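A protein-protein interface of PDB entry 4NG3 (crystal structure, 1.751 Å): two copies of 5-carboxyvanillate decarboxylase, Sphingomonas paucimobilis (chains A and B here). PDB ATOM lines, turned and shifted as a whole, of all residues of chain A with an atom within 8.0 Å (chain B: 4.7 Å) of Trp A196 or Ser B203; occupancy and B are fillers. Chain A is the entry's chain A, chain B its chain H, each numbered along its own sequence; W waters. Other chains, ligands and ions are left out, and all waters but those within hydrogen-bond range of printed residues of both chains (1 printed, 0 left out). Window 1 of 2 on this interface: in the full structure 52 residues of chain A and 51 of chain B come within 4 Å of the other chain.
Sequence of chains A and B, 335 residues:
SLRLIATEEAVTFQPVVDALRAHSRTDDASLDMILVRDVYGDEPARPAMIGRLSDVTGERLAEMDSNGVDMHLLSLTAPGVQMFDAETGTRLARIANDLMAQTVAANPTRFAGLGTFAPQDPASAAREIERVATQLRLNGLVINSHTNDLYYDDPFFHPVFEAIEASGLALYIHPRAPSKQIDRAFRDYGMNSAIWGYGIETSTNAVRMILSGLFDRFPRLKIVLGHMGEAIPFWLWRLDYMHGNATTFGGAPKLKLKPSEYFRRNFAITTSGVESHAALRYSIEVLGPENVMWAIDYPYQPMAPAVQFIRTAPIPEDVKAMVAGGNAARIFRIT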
ATOM      1  N   ARG A 176     -13.491  18.509 -15.935  1.00  0.00           N
ATOM      2  CA  ARG A 176     -14.330  18.185 -17.085  1.00  0.00           C
ATOM      3  C   ARG A 176     -13.836  19.139 -18.176  1.00  0.00           C
ATOM      4  O   ARG A 176     -12.926  19.943 -17.923  1.00  0.00           O
ATOM      5  CB  ARG A 176     -15.819  18.383 -16.787  1.00  0.00           C
ATOM      6  CG  ARG A 176     -16.219  19.807 -16.451  1.00  0.00           C
ATOM      7  CD  ARG A 176     -17.723  19.940 -16.193  1.00  0.00           C
ATOM      8  NE  ARG A 176     -18.530  19.731 -17.392  1.00  0.00           N
ATOM      9  CZ  ARG A 176     -19.830  19.998 -17.470  1.00  0.00           C
ATOM     10  NH1 ARG A 176     -20.475  20.480 -16.412  1.00  0.00           N
ATOM     11  NH2 ARG A 176     -20.486  19.784 -18.603  1.00  0.00           N
ATOM     12  N   PRO A 178     -13.353  22.283 -20.599  1.00  0.00           N
ATOM     13  CA  PRO A 178     -13.531  23.732 -20.486  1.00  0.00           C
ATOM     14  C   PRO A 178     -14.978  24.158 -20.692  1.00  0.00           C
ATOM     15  O   PRO A 178     -15.631  23.734 -21.647  1.00  0.00           O
ATOM     16  CB  PRO A 178     -12.674  24.249 -21.634  1.00  0.00           C
ATOM     17  CG  PRO A 178     -11.491  23.321 -21.593  1.00  0.00           C
ATOM     18  CD  PRO A 178     -12.084  21.949 -21.273  1.00  0.00           C
ATOM     19  N   ILE A 182     -14.810  29.454 -21.770  1.00  0.00           N
ATOM     20  CA  ILE A 182     -13.465  29.337 -22.325  1.00  0.00           C
ATOM     21  C   ILE A 182     -13.314  28.333 -23.475  1.00  0.00           C
ATOM     22  O   ILE A 182     -12.237  28.237 -24.072  1.00  0.00           O
ATOM     23  CB  ILE A 182     -12.439  28.982 -21.234  1.00  0.00           C
ATOM     24  CG1 ILE A 182     -12.801  27.659 -20.565  1.00  0.00           C
ATOM     25  CG2 ILE A 182     -12.366  30.051 -20.164  1.00  0.00           C
ATOM     26  CD1 ILE A 182     -11.744  27.196 -19.599  1.00  0.00           C
ATOM     27  N   ALA A 185     -11.246  28.152 -27.341  1.00  0.00           N
ATOM     28  CA  ALA A 185      -9.812  27.957 -27.531  1.00  0.00           C
ATOM     29  C   ALA A 185      -9.362  26.495 -27.399  1.00  0.00           C
ATOM     30  O   ALA A 185      -8.168  26.195 -27.527  1.00  0.00           O
ATOM     31  CB  ALA A 185      -9.032  28.848 -26.551  1.00  0.00           C
ATOM     32  N   PHE A 186     -10.312  25.588 -27.160  1.00  0.00           N
ATOM     33  CA  PHE A 186      -9.968  24.201 -26.871  1.00  0.00           C
ATOM     34  C   PHE A 186     -10.620  23.210 -27.827  1.00  0.00           C
ATOM     35  O   PHE A 186     -10.784  22.039 -27.496  1.00  0.00           O
ATOM     36  CB  PHE A 186     -10.339  23.858 -25.428  1.00  0.00           C
ATOM     37  CG  PHE A 186      -9.636  24.719 -24.410  1.00  0.00           C
ATOM     38  CD1 PHE A 186     -10.151  25.955 -24.049  1.00  0.00           C
ATOM     39  CD2 PHE A 186      -8.462  24.293 -23.818  1.00  0.00           C
ATOM     40  CE1 PHE A 186      -9.504  26.752 -23.128  1.00  0.00           C
ATOM     41  CE2 PHE A 186      -7.808  25.086 -22.885  1.00  0.00           C
ATOM     42  CZ  PHE A 186      -8.332  26.316 -22.538  1.00  0.00           C
ATOM     43  N   ASP A 188      -9.435  22.421 -30.802  1.00  0.00           N
ATOM     44  CA  ASP A 188      -8.450  21.885 -31.740  1.00  0.00           C
ATOM     45  C   ASP A 188      -7.401  21.002 -31.078  1.00  0.00           C
ATOM     46  O   ASP A 188      -7.101  21.158 -29.895  1.00  0.00           O
ATOM     47  CB  ASP A 188      -7.763  23.034 -32.477  1.00  0.00           C
ATOM     48  CG  ASP A 188      -8.745  23.897 -33.246  1.00  0.00           C
ATOM     49  OD1 ASP A 188      -9.477  23.337 -34.086  1.00  0.00           O
ATOM     50  OD2 ASP A 188      -8.800  25.122 -33.000  1.00  0.00           O
ATOM     51  N   TYR A 189      -6.849  20.077 -31.859  1.00  0.00           N
ATOM     52  CA  TYR A 189      -5.733  19.228 -31.427  1.00  0.00           C
ATOM     53  C   TYR A 189      -6.006  18.382 -30.172  1.00  0.00           C
ATOM     54  O   TYR A 189      -5.083  18.055 -29.426  1.00  0.00           O
ATOM     55  CB  TYR A 189      -4.474  20.079 -31.225  1.00  0.00           C
ATOM     56  CG  TYR A 189      -4.336  21.199 -32.238  1.00  0.00           C
ATOM     57  CD1 TYR A 189      -4.277  20.923 -33.602  1.00  0.00           C
ATOM     58  CD2 TYR A 189      -4.267  22.529 -31.833  1.00  0.00           C
ATOM     59  CE1 TYR A 189      -4.147  21.941 -34.537  1.00  0.00           C
ATOM     60  CE2 TYR A 189      -4.144  23.556 -32.773  1.00  0.00           C
ATOM     61  CZ  TYR A 189      -4.091  23.244 -34.118  1.00  0.00           C
ATOM     62  OH  TYR A 189      -3.969  24.238 -35.060  1.00  0.00           O
ATOM     63  N   GLY A 190      -7.269  18.031 -29.944  1.00  0.00           N
ATOM     64  CA  GLY A 190      -7.650  17.242 -28.785  1.00  0.00           C
ATOM     65  C   GLY A 190      -7.521  17.982 -27.462  1.00  0.00           C
ATOM     66  O   GLY A 190      -7.527  17.384 -26.379  1.00  0.00           O
ATOM     67  N   MET A 191      -7.420  19.301 -27.539  1.00  0.00           N
ATOM     68  CA  MET A 191      -7.176  20.093 -26.343  1.00  0.00           C
ATOM     69  C   MET A 191      -8.392  20.214 -25.410  1.00  0.00           C
ATOM     70  O   MET A 191      -8.282  20.747 -24.309  1.00  0.00           O
ATOM     71  CB  MET A 191      -6.627  21.471 -26.713  1.00  0.00           C
ATOM     72  CG  MET A 191      -5.222  21.392 -27.284  1.00  0.00           C
ATOM     73  SD  MET A 191      -4.678  22.978 -27.920  1.00  0.00           S
ATOM     74  CE  MET A 191      -4.768  23.963 -26.427  1.00  0.00           C
ATOM     75  N   ASN A 192      -9.542  19.717 -25.846  1.00  0.00           N
ATOM     76  CA  ASN A 192     -10.703  19.639 -24.963  1.00  0.00           C
ATOM     77  C   ASN A 192     -10.445  18.789 -23.728  1.00  0.00           C
ATOM     78  O   ASN A 192     -11.092  18.966 -22.684  1.00  0.00           O
ATOM     79  CB  ASN A 192     -11.917  19.063 -25.709  1.00  0.00           C
ATOM     80  CG  ASN A 192     -11.825  17.549 -25.915  1.00  0.00           C
ATOM     81  OD1 ASN A 192     -12.262  16.764 -25.065  1.00  0.00           O
ATOM     82  ND2 ASN A 192     -11.274  17.138 -27.049  1.00  0.00           N
ATOM     83  N   SER A 193      -9.498  17.865 -23.850  1.00  0.00           N
ATOM     84  CA  SER A 193      -9.363  16.773 -22.891  1.00  0.00           C
ATOM     85  C   SER A 193      -8.200  16.945 -21.917  1.00  0.00           C
ATOM     86  O   SER A 193      -7.751  18.065 -21.631  1.00  0.00           O
ATOM     87  CB  SER A 193      -9.237  15.444 -23.667  1.00  0.00           C
ATOM     88  OG  SER A 193      -9.346  14.301 -22.819  1.00  0.00           O
ATOM     89  N   ALA A 194      -7.718  15.819 -21.403  1.00  0.00           N
ATOM     90  CA  ALA A 194      -6.673  15.804 -20.378  1.00  0.00           C
ATOM     91  C   ALA A 194      -5.356  16.454 -20.792  1.00  0.00           C
ATOM     92  O   ALA A 194      -4.610  16.964 -19.941  1.00  0.00           O
ATOM     93  CB  ALA A 194      -6.425  14.372 -19.931  1.00  0.00           C
ATOM     94  N   ILE A 195      -5.067  16.446 -22.088  1.00  0.00           N
ATOM     95  CA  ILE A 195      -3.820  17.023 -22.575  1.00  0.00           C
ATOM     96  C   ILE A 195      -3.650  18.512 -22.235  1.00  0.00           C
ATOM     97  O   ILE A 195      -2.532  18.966 -22.047  1.00  0.00           O
ATOM     98  CB  ILE A 195      -3.591  16.754 -24.087  1.00  0.00           C
ATOM     99  CG1 ILE A 195      -2.112  16.943 -24.439  1.00  0.00           C
ATOM    100  CG2 ILE A 195      -4.493  17.626 -24.945  1.00  0.00           C
ATOM    101  CD1 ILE A 195      -1.753  16.576 -25.867  1.00  0.00           C
ATOM    102  N   TRP A 196      -4.744  19.265 -22.128  1.00  0.00           N
ATOM    103  CA  TRP A 196      -4.625  20.683 -21.774  1.00  0.00           C
ATOM    104  C   TRP A 196      -5.876  21.300 -21.149  1.00  0.00           C
ATOM    105  O   TRP A 196      -5.798  21.931 -20.087  1.00  0.00           O
ATOM    106  CB  TRP A 196      -4.185  21.525 -22.985  1.00  0.00           C
ATOM    107  CG  TRP A 196      -3.707  22.894 -22.589  1.00  0.00           C
ATOM    108  CD1 TRP A 196      -4.256  24.103 -22.949  1.00  0.00           C
ATOM    109  CD2 TRP A 196      -2.592  23.198 -21.743  1.00  0.00           C
ATOM    110  NE1 TRP A 196      -3.536  25.136 -22.385  1.00  0.00           N
ATOM    111  CE2 TRP A 196      -2.514  24.606 -21.638  1.00  0.00           C
ATOM    112  CE3 TRP A 196      -1.642  22.416 -21.077  1.00  0.00           C
ATOM    113  CZ2 TRP A 196      -1.529  25.245 -20.886  1.00  0.00           C
ATOM    114  CZ3 TRP A 196      -0.666  23.052 -20.333  1.00  0.00           C
ATOM    115  CH2 TRP A 196      -0.617  24.451 -20.243  1.00  0.00           C
ATOM    116  N   GLY A 197      -7.022  21.136 -21.812  1.00  0.00           N
ATOM    117  CA  GLY A 197      -8.253  21.741 -21.345  1.00  0.00           C
ATOM    118  C   GLY A 197      -8.680  21.384 -19.932  1.00  0.00           C
ATOM    119  O   GLY A 197      -9.134  22.254 -19.196  1.00  0.00           O
ATOM    120  N   TYR A 198      -8.538  20.117 -19.548  1.00  0.00           N
ATOM    121  CA  TYR A 198      -8.947  19.693 -18.211  1.00  0.00           C
ATOM    122  C   TYR A 198      -8.235  20.511 -17.129  1.00  0.00           C
ATOM    123  O   TYR A 198      -8.851  20.953 -16.165  1.00  0.00           O
ATOM    124  CB  TYR A 198      -8.672  18.200 -17.988  1.00  0.00           C
ATOM    125  CG  TYR A 198      -9.725  17.267 -18.557  1.00  0.00           C
ATOM    126  CD1 TYR A 198     -10.738  17.742 -19.382  1.00  0.00           C
ATOM    127  CD2 TYR A 198      -9.727  15.910 -18.232  1.00  0.00           C
ATOM    128  CE1 TYR A 198     -11.721  16.887 -19.895  1.00  0.00           C
ATOM    129  CE2 TYR A 198     -10.700  15.049 -18.745  1.00  0.00           C
ATOM    130  CZ  TYR A 198     -11.687  15.546 -19.579  1.00  0.00           C
ATOM    131  OH  TYR A 198     -12.655  14.704 -20.088  1.00  0.00           O
ATOM    132  N   GLY A 199      -6.937  20.714 -17.297  1.00  0.00           N
ATOM    133  CA  GLY A 199      -6.160  21.440 -16.305  1.00  0.00           C
ATOM    134  C   GLY A 199      -6.510  22.920 -16.212  1.00  0.00           C
ATOM    135  O   GLY A 199      -6.598  23.490 -15.119  1.00  0.00           O
ATOM    136  N   ILE A 200      -6.689  23.549 -17.361  1.00  0.00           N
ATOM    137  CA  ILE A 200      -6.963  24.980 -17.404  1.00  0.00           C
ATOM    138  C   ILE A 200      -8.336  25.246 -16.796  1.00  0.00           C
ATOM    139  O   ILE A 200      -8.512  26.145 -15.976  1.00  0.00           O
ATOM    140  CB  ILE A 200      -6.924  25.498 -18.850  1.00  0.00           C
ATOM    141  CG1 ILE A 200      -5.534  25.272 -19.455  1.00  0.00           C
ATOM    142  CG2 ILE A 200      -7.366  26.965 -18.923  1.00  0.00           C
ATOM    143  CD1 ILE A 200      -4.385  25.662 -18.522  1.00  0.00           C
ATOM    144  N   GLU A 201      -9.307  24.447 -17.210  1.00  0.00           N
ATOM    145  CA  GLU A 201     -10.665  24.530 -16.689  1.00  0.00           C
ATOM    146  C   GLU A 201     -10.702  24.386 -15.171  1.00  0.00           C
ATOM    147  O   GLU A 201     -11.350  25.179 -14.476  1.00  0.00           O
ATOM    148  CB  GLU A 201     -11.536  23.462 -17.384  1.00  0.00           C
ATOM    149  CG  GLU A 201     -12.800  23.039 -16.644  1.00  0.00           C
ATOM    150  CD  GLU A 201     -13.820  24.140 -16.524  1.00  0.00           C
ATOM    151  OE1 GLU A 201     -13.784  25.106 -17.327  1.00  0.00           O
ATOM    152  OE2 GLU A 201     -14.662  24.045 -15.604  1.00  0.00           O
ATOM    153  N   THR A 202      -9.990  23.388 -14.644  1.00  0.00           N
ATOM    154  CA  THR A 202     -10.118  23.047 -13.234  1.00  0.00           C
ATOM    155  C   THR A 202      -9.317  24.013 -12.352  1.00  0.00           C
ATOM    156  O   THR A 202      -9.790  24.456 -11.307  1.00  0.00           O
ATOM    157  CB  THR A 202      -9.679  21.591 -12.985  1.00  0.00           C
ATOM    158  OG1 THR A 202     -10.352  20.734 -13.923  1.00  0.00           O
ATOM    159  CG2 THR A 202     -10.013  21.166 -11.570  1.00  0.00           C
ATOM    160  N   SER A 203      -8.113  24.361 -12.796  1.00  0.00           N
ATOM    161  CA  SER A 203      -7.264  25.292 -12.057  1.00  0.00           C
ATOM    162  C   SER A 203      -7.902  26.677 -12.021  1.00  0.00           C
ATOM    163  O   SER A 203      -7.818  27.371 -11.010  1.00  0.00           O
ATOM    164  CB  SER A 203      -5.858  25.358 -12.667  1.00  0.00           C
ATOM    165  OG  SER A 203      -5.887  25.854 -13.995  1.00  0.00           O
ATOM    166  N   GLU A 230      -3.317  20.522 -10.547  1.00  0.00           N
ATOM    167  CA  GLU A 230      -3.636  21.270 -11.766  1.00  0.00           C
ATOM    168  C   GLU A 230      -2.669  22.450 -11.957  1.00  0.00           C
ATOM    169  O   GLU A 230      -3.054  23.537 -12.425  1.00  0.00           O
ATOM    170  CB  GLU A 230      -5.110  21.723 -11.779  1.00  0.00           C
ATOM    171  CG  GLU A 230      -6.153  20.609 -11.449  1.00  0.00           C
ATOM    172  CD  GLU A 230      -6.276  19.531 -12.525  1.00  0.00           C
ATOM    173  OE1 GLU A 230      -5.597  19.643 -13.565  1.00  0.00           O
ATOM    174  OE2 GLU A 230      -7.061  18.568 -12.329  1.00  0.00           O
ATOM    175  N   ALA A 231      -1.416  22.204 -11.568  1.00  0.00           N
ATOM    176  CA  ALA A 231      -0.301  23.145 -11.677  1.00  0.00           C
ATOM    177  C   ALA A 231      -0.361  24.349 -10.751  1.00  0.00           C
ATOM    178  O   ALA A 231       0.549  25.171 -10.764  1.00  0.00           O
ATOM    179  CB  ALA A 231      -0.088  23.603 -13.140  1.00  0.00           C
ATOM    180  N   TRP A 235       2.395  27.849  -9.469  1.00  0.00           N
ATOM    181  CA  TRP A 235       2.058  29.273  -9.596  1.00  0.00           C
ATOM    182  C   TRP A 235       1.972  30.016  -8.265  1.00  0.00           C
ATOM    183  O   TRP A 235       1.598  31.183  -8.239  1.00  0.00           O
ATOM    184  CB  TRP A 235       0.700  29.455 -10.288  1.00  0.00           C
ATOM    185  CG  TRP A 235       0.620  29.160 -11.760  1.00  0.00           C
ATOM    186  CD1 TRP A 235       0.039  28.069 -12.340  1.00  0.00           C
ATOM    187  CD2 TRP A 235       1.072  29.994 -12.840  1.00  0.00           C
ATOM    188  NE1 TRP A 235       0.121  28.157 -13.699  1.00  0.00           N
ATOM    189  CE2 TRP A 235       0.747  29.330 -14.038  1.00  0.00           C
ATOM    190  CE3 TRP A 235       1.734  31.228 -12.906  1.00  0.00           C
ATOM    191  CZ2 TRP A 235       1.059  29.855 -15.296  1.00  0.00           C
ATOM    192  CZ3 TRP A 235       2.045  31.752 -14.151  1.00  0.00           C
ATOM    193  CH2 TRP A 235       1.701  31.064 -15.335  1.00  0.00           C
ATOM    194  N   GLY B 199      -0.951  34.128 -17.657  1.00  0.00           N
ATOM    195  CA  GLY B 199      -0.372  32.801 -17.774  1.00  0.00           C
ATOM    196  C   GLY B 199      -1.215  31.845 -18.598  1.00  0.00           C
ATOM    197  O   GLY B 199      -0.691  31.117 -19.435  1.00  0.00           O
ATOM    198  N   ILE B 200      -2.520  31.823 -18.352  1.00  0.00           N
ATOM    199  CA  ILE B 200      -3.411  30.932 -19.099  1.00  0.00           C
ATOM    200  C   ILE B 200      -3.431  31.282 -20.588  1.00  0.00           C
ATOM    201  O   ILE B 200      -3.346  30.407 -21.451  1.00  0.00           O
ATOM    202  CB  ILE B 200      -4.853  30.970 -18.538  1.00  0.00           C
ATOM    203  CG1 ILE B 200      -4.881  30.576 -17.058  1.00  0.00           C
ATOM    204  CG2 ILE B 200      -5.774  30.064 -19.351  1.00  0.00           C
ATOM    205  CD1 ILE B 200      -4.289  29.199 -16.761  1.00  0.00           C
ATOM    206  N   GLU B 201      -3.538  32.571 -20.886  1.00  0.00           N
ATOM    207  CA  GLU B 201      -3.541  33.053 -22.260  1.00  0.00           C
ATOM    208  C   GLU B 201      -2.275  32.666 -23.019  1.00  0.00           C
ATOM    209  O   GLU B 201      -2.336  32.154 -24.139  1.00  0.00           O
ATOM    210  CB  GLU B 201      -3.690  34.580 -22.252  1.00  0.00           C
ATOM    211  CG  GLU B 201      -3.191  35.278 -23.504  1.00  0.00           C
ATOM    212  CD  GLU B 201      -4.021  34.970 -24.733  1.00  0.00           C
ATOM    213  OE1 GLU B 201      -5.154  34.446 -24.598  1.00  0.00           O
ATOM    214  OE2 GLU B 201      -3.537  35.261 -25.847  1.00  0.00           O
ATOM    215  N   THR B 202      -1.128  32.910 -22.401  1.00  0.00           N
ATOM    216  CA  THR B 202       0.152  32.735 -23.076  1.00  0.00           C
ATOM    217  C   THR B 202       0.514  31.262 -23.165  1.00  0.00           C
ATOM    218  O   THR B 202       0.965  30.782 -24.207  1.00  0.00           O
ATOM    219  CB  THR B 202       1.272  33.519 -22.359  1.00  0.00           C
ATOM    220  OG1 THR B 202       0.846  34.871 -22.167  1.00  0.00           O
ATOM    221  CG2 THR B 202       2.545  33.529 -23.199  1.00  0.00           C
ATOM    222  N   SER B 203       0.298  30.530 -22.083  1.00  0.00           N
ATOM    223  CA  SER B 203       0.610  29.108 -22.114  1.00  0.00           C
ATOM    224  C   SER B 203      -0.269  28.386 -23.141  1.00  0.00           C
ATOM    225  O   SER B 203       0.196  27.490 -23.837  1.00  0.00           O
ATOM    226  CB  SER B 203       0.452  28.476 -20.731  1.00  0.00           C
ATOM    227  OG  SER B 203      -0.893  28.558 -20.286  1.00  0.00           O
ATOM    228  N   THR B 204      -1.534  28.791 -23.248  1.00  0.00           N
ATOM    229  CA  THR B 204      -2.453  28.116 -24.167  1.00  0.00           C
ATOM    230  C   THR B 204      -2.052  28.383 -25.610  1.00  0.00           C
ATOM    231  O   THR B 204      -2.133  27.498 -26.459  1.00  0.00           O
ATOM    232  CB  THR B 204      -3.912  28.510 -23.893  1.00  0.00           C
ATOM    233  OG1 THR B 204      -4.282  28.043 -22.590  1.00  0.00           O
ATOM    234  CG2 THR B 204      -4.858  27.891 -24.933  1.00  0.00           C
ATOM    235  N   ASN B 205      -1.588  29.604 -25.873  1.00  0.00           N
ATOM    236  CA  ASN B 205      -1.045  29.967 -27.179  1.00  0.00           C
ATOM    237  C   ASN B 205       0.103  29.017 -27.523  1.00  0.00           C
ATOM    238  O   ASN B 205       0.101  28.368 -28.572  1.00  0.00           O
ATOM    239  CB  ASN B 205      -0.565  31.424 -27.137  1.00  0.00           C
ATOM    240  CG  ASN B 205      -0.375  32.037 -28.517  1.00  0.00           C
ATOM    241  OD1 ASN B 205      -0.313  31.339 -29.530  1.00  0.00           O
ATOM    242  ND2 ASN B 205      -0.279  33.369 -28.557  1.00  0.00           N
ATOM    243  N   ALA B 206       1.066  28.922 -26.611  1.00  0.00           N
ATOM    244  CA  ALA B 206       2.267  28.121 -26.817  1.00  0.00           C
ATOM    245  C   ALA B 206       1.945  26.639 -27.037  1.00  0.00           C
ATOM    246  O   ALA B 206       2.523  25.984 -27.904  1.00  0.00           O
ATOM    247  CB  ALA B 206       3.217  28.303 -25.619  1.00  0.00           C
ATOM    248  N   VAL B 207       1.015  26.112 -26.249  1.00  0.00           N
ATOM    249  CA  VAL B 207       0.606  24.720 -26.392  1.00  0.00           C
ATOM    250  C   VAL B 207      -0.058  24.481 -27.754  1.00  0.00           C
ATOM    251  O   VAL B 207       0.211  23.472 -28.398  1.00  0.00           O
ATOM    252  CB  VAL B 207      -0.294  24.271 -25.224  1.00  0.00           C
ATOM    253  CG1 VAL B 207      -0.900  22.891 -25.500  1.00  0.00           C
ATOM    254  CG2 VAL B 207       0.524  24.251 -23.927  1.00  0.00           C
ATOM    255  N   GLU B 230       5.503  30.065 -18.175  1.00  0.00           N
ATOM    256  CA  GLU B 230       4.041  30.074 -18.048  1.00  0.00           C
ATOM    257  C   GLU B 230       3.517  28.711 -17.610  1.00  0.00           C
ATOM    258  O   GLU B 230       2.480  28.238 -18.092  1.00  0.00           O
ATOM    259  CB  GLU B 230       3.371  30.515 -19.351  1.00  0.00           C
ATOM    260  CG  GLU B 230       3.976  31.788 -19.979  1.00  0.00           C
ATOM    261  CD  GLU B 230       3.669  33.079 -19.206  1.00  0.00           C
ATOM    262  OE1 GLU B 230       2.946  33.025 -18.188  1.00  0.00           O
ATOM    263  OE2 GLU B 230       4.156  34.159 -19.629  1.00  0.00           O
ATOM    264  N   ILE B 232       4.315  25.775 -18.285  1.00  0.00           N
ATOM    265  CA  ILE B 232       4.455  24.629 -19.189  1.00  0.00           C
ATOM    266  C   ILE B 232       5.510  23.593 -18.714  1.00  0.00           C
ATOM    267  O   ILE B 232       5.282  22.383 -18.835  1.00  0.00           O
ATOM    268  CB  ILE B 232       4.678  25.080 -20.657  1.00  0.00           C
ATOM    269  CG1 ILE B 232       3.421  25.803 -21.171  1.00  0.00           C
ATOM    270  CG2 ILE B 232       4.999  23.872 -21.552  1.00  0.00           C
ATOM    271  CD1 ILE B 232       3.595  26.500 -22.522  1.00  0.00           C
ATOM    272  N   TRP B 235       3.924  20.916 -16.721  1.00  0.00           N
ATOM    273  CA  TRP B 235       2.945  20.066 -17.383  1.00  0.00           C
ATOM    274  C   TRP B 235       3.567  19.098 -18.390  1.00  0.00           C
ATOM    275  O   TRP B 235       2.846  18.458 -19.142  1.00  0.00           O
ATOM    276  CB  TRP B 235       1.951  20.944 -18.162  1.00  0.00           C
ATOM    277  CG  TRP B 235       0.900  21.664 -17.359  1.00  0.00           C
ATOM    278  CD1 TRP B 235       0.830  23.014 -17.119  1.00  0.00           C
ATOM    279  CD2 TRP B 235      -0.259  21.085 -16.735  1.00  0.00           C
ATOM    280  NE1 TRP B 235      -0.296  23.301 -16.377  1.00  0.00           N
ATOM    281  CE2 TRP B 235      -0.974  22.134 -16.124  1.00  0.00           C
ATOM    282  CE3 TRP B 235      -0.752  19.775 -16.621  1.00  0.00           C
ATOM    283  CZ2 TRP B 235      -2.163  21.917 -15.410  1.00  0.00           C
ATOM    284  CZ3 TRP B 235      -1.926  19.562 -15.909  1.00  0.00           C
ATOM    285  CH2 TRP B 235      -2.621  20.629 -15.321  1.00  0.00           C
ATOM    286  N   LEU B 239       1.505  16.430 -20.896  1.00  0.00           N
ATOM    287  CA  LEU B 239       1.488  16.789 -22.314  1.00  0.00           C
ATOM    288  C   LEU B 239       1.966  15.629 -23.180  1.00  0.00           C
ATOM    289  O   LEU B 239       1.333  15.284 -24.184  1.00  0.00           O
ATOM    290  CB  LEU B 239       2.346  18.040 -22.586  1.00  0.00           C
ATOM    291  CG  LEU B 239       1.742  19.405 -22.195  1.00  0.00           C
ATOM    292  CD1 LEU B 239       2.806  20.511 -22.149  1.00  0.00           C
ATOM    293  CD2 LEU B 239       0.612  19.799 -23.157  1.00  0.00           C
HETATM  294  O   HOH W   1      -0.872  26.130 -15.642  1.00  0.00           O
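The side-chain hydroxyl of Ser A203 lies within hydrogen-bond range of the backbone carbonyl oxygen of Gly A199 (2.7 Å). The backbone carbonyl oxygen (O) of Ile A200 sits at hydrogen-bond distance from the side-chain hydroxyl (OG) of Ser A203. The side-chain hydroxyl (OG) of Ser B203 lies within hydrogen-bond range of the backbone carbonyl oxygen (O) of Gly B199, at 2.7 Å. The side-chain hydroxyl of Ser B203 sits at hydrogen-bond distance from the backbone carbonyl oxygen of Ile B200, at 3.3 Å. O of Ile B200 sits at hydrogen-bond distance from OG1 of Thr B204.
Among the printed residues, pairs that only touch across the chains: Ile A195 with Leu B239, Trp A196 with Ser B203, Trp A196 with Val B207, Trp A196 with Trp B235, Gly A199 with Trp B235, Ile A200 with Ile B200, Glu A230 with Trp B235, Ala A231 with Trp B235, Trp A235 with Gly B199 and Trp A235 with Glu B230.
Ile A182 touches none of the printed residues of chain B. Of the printed residues of chain B, Ile A195 touches Leu B239 (3.4 Å). Of chain B, only Ser B203, Thr B204, Val B207 and Trp B235 come within 4 Å of Trp A196. Of the printed residues of chain B, Ile A200 touches Ile B200. Printed residues of chain B within 4 Å of Glu A230: Trp B235. Of chain A, only Trp A196 comes within 4 Å of Ser B203. Printed residues of chain A within 4 Å of Val B207: Trp A196. Printed residues of chain A within 4 Å of Leu B239: Ile A195 (3.4 Å). The nearest residue of chain A that does not touch Ser B203 is Ile A200 (4.9 Å).
Water W1 lies within hydrogen-bond range of the indole nitrogen (NE1) of Trp A235 (3.0 Å) and the indole nitrogen (NE1) of Trp B235 (3.0 Å).
Of the 24 printed residues of chain A, 7 touch a printed residue of chain B. Printed residues of chain A that touch a printed residue of chain B: Ile A195, Trp A196, Gly A199, Ile A200, Glu A230, Ala A231 and Trp A235. Of the 13 printed residues of chain B, 8 touch a printed residue of chain A. Printed residues of chain B that touch a printed residue of chain A: Gly B199, Ile B200, Ser B203, Thr B204, Val B207, Glu B230, Trp B235 and Leu B239. Hydrophobic or aromatic side chains of chain B within 4 Å of the printed part of chain A: Ile B200, Val B207, Trp B235 and Leu B239. Among the printed residues, no Asp or Glu carboxylate lies within 4 Å of a Lys or Arg side-chain nitrogen of the other chain.
The indole nitrogen of Trp A196 is in hydrogen-bond range of the side-chain hydroxyl of Thr B204, 3.0 Å away.
Gly A199 touches Trp B235, and with the chains exchanged Trp A235 touches Gly B199. Ile B200 touches its own counterpart, Ile A200. Glu A230 touches Trp B235, and with the chains exchanged Trp A235 touches Glu B230. Positions printed for both chains: 199, 200, 201, 202, 203, 230 and 235. Of the 11 pairs that touch across the chains among the printed residues, 5 have their exchanged pair printed and touching as well.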
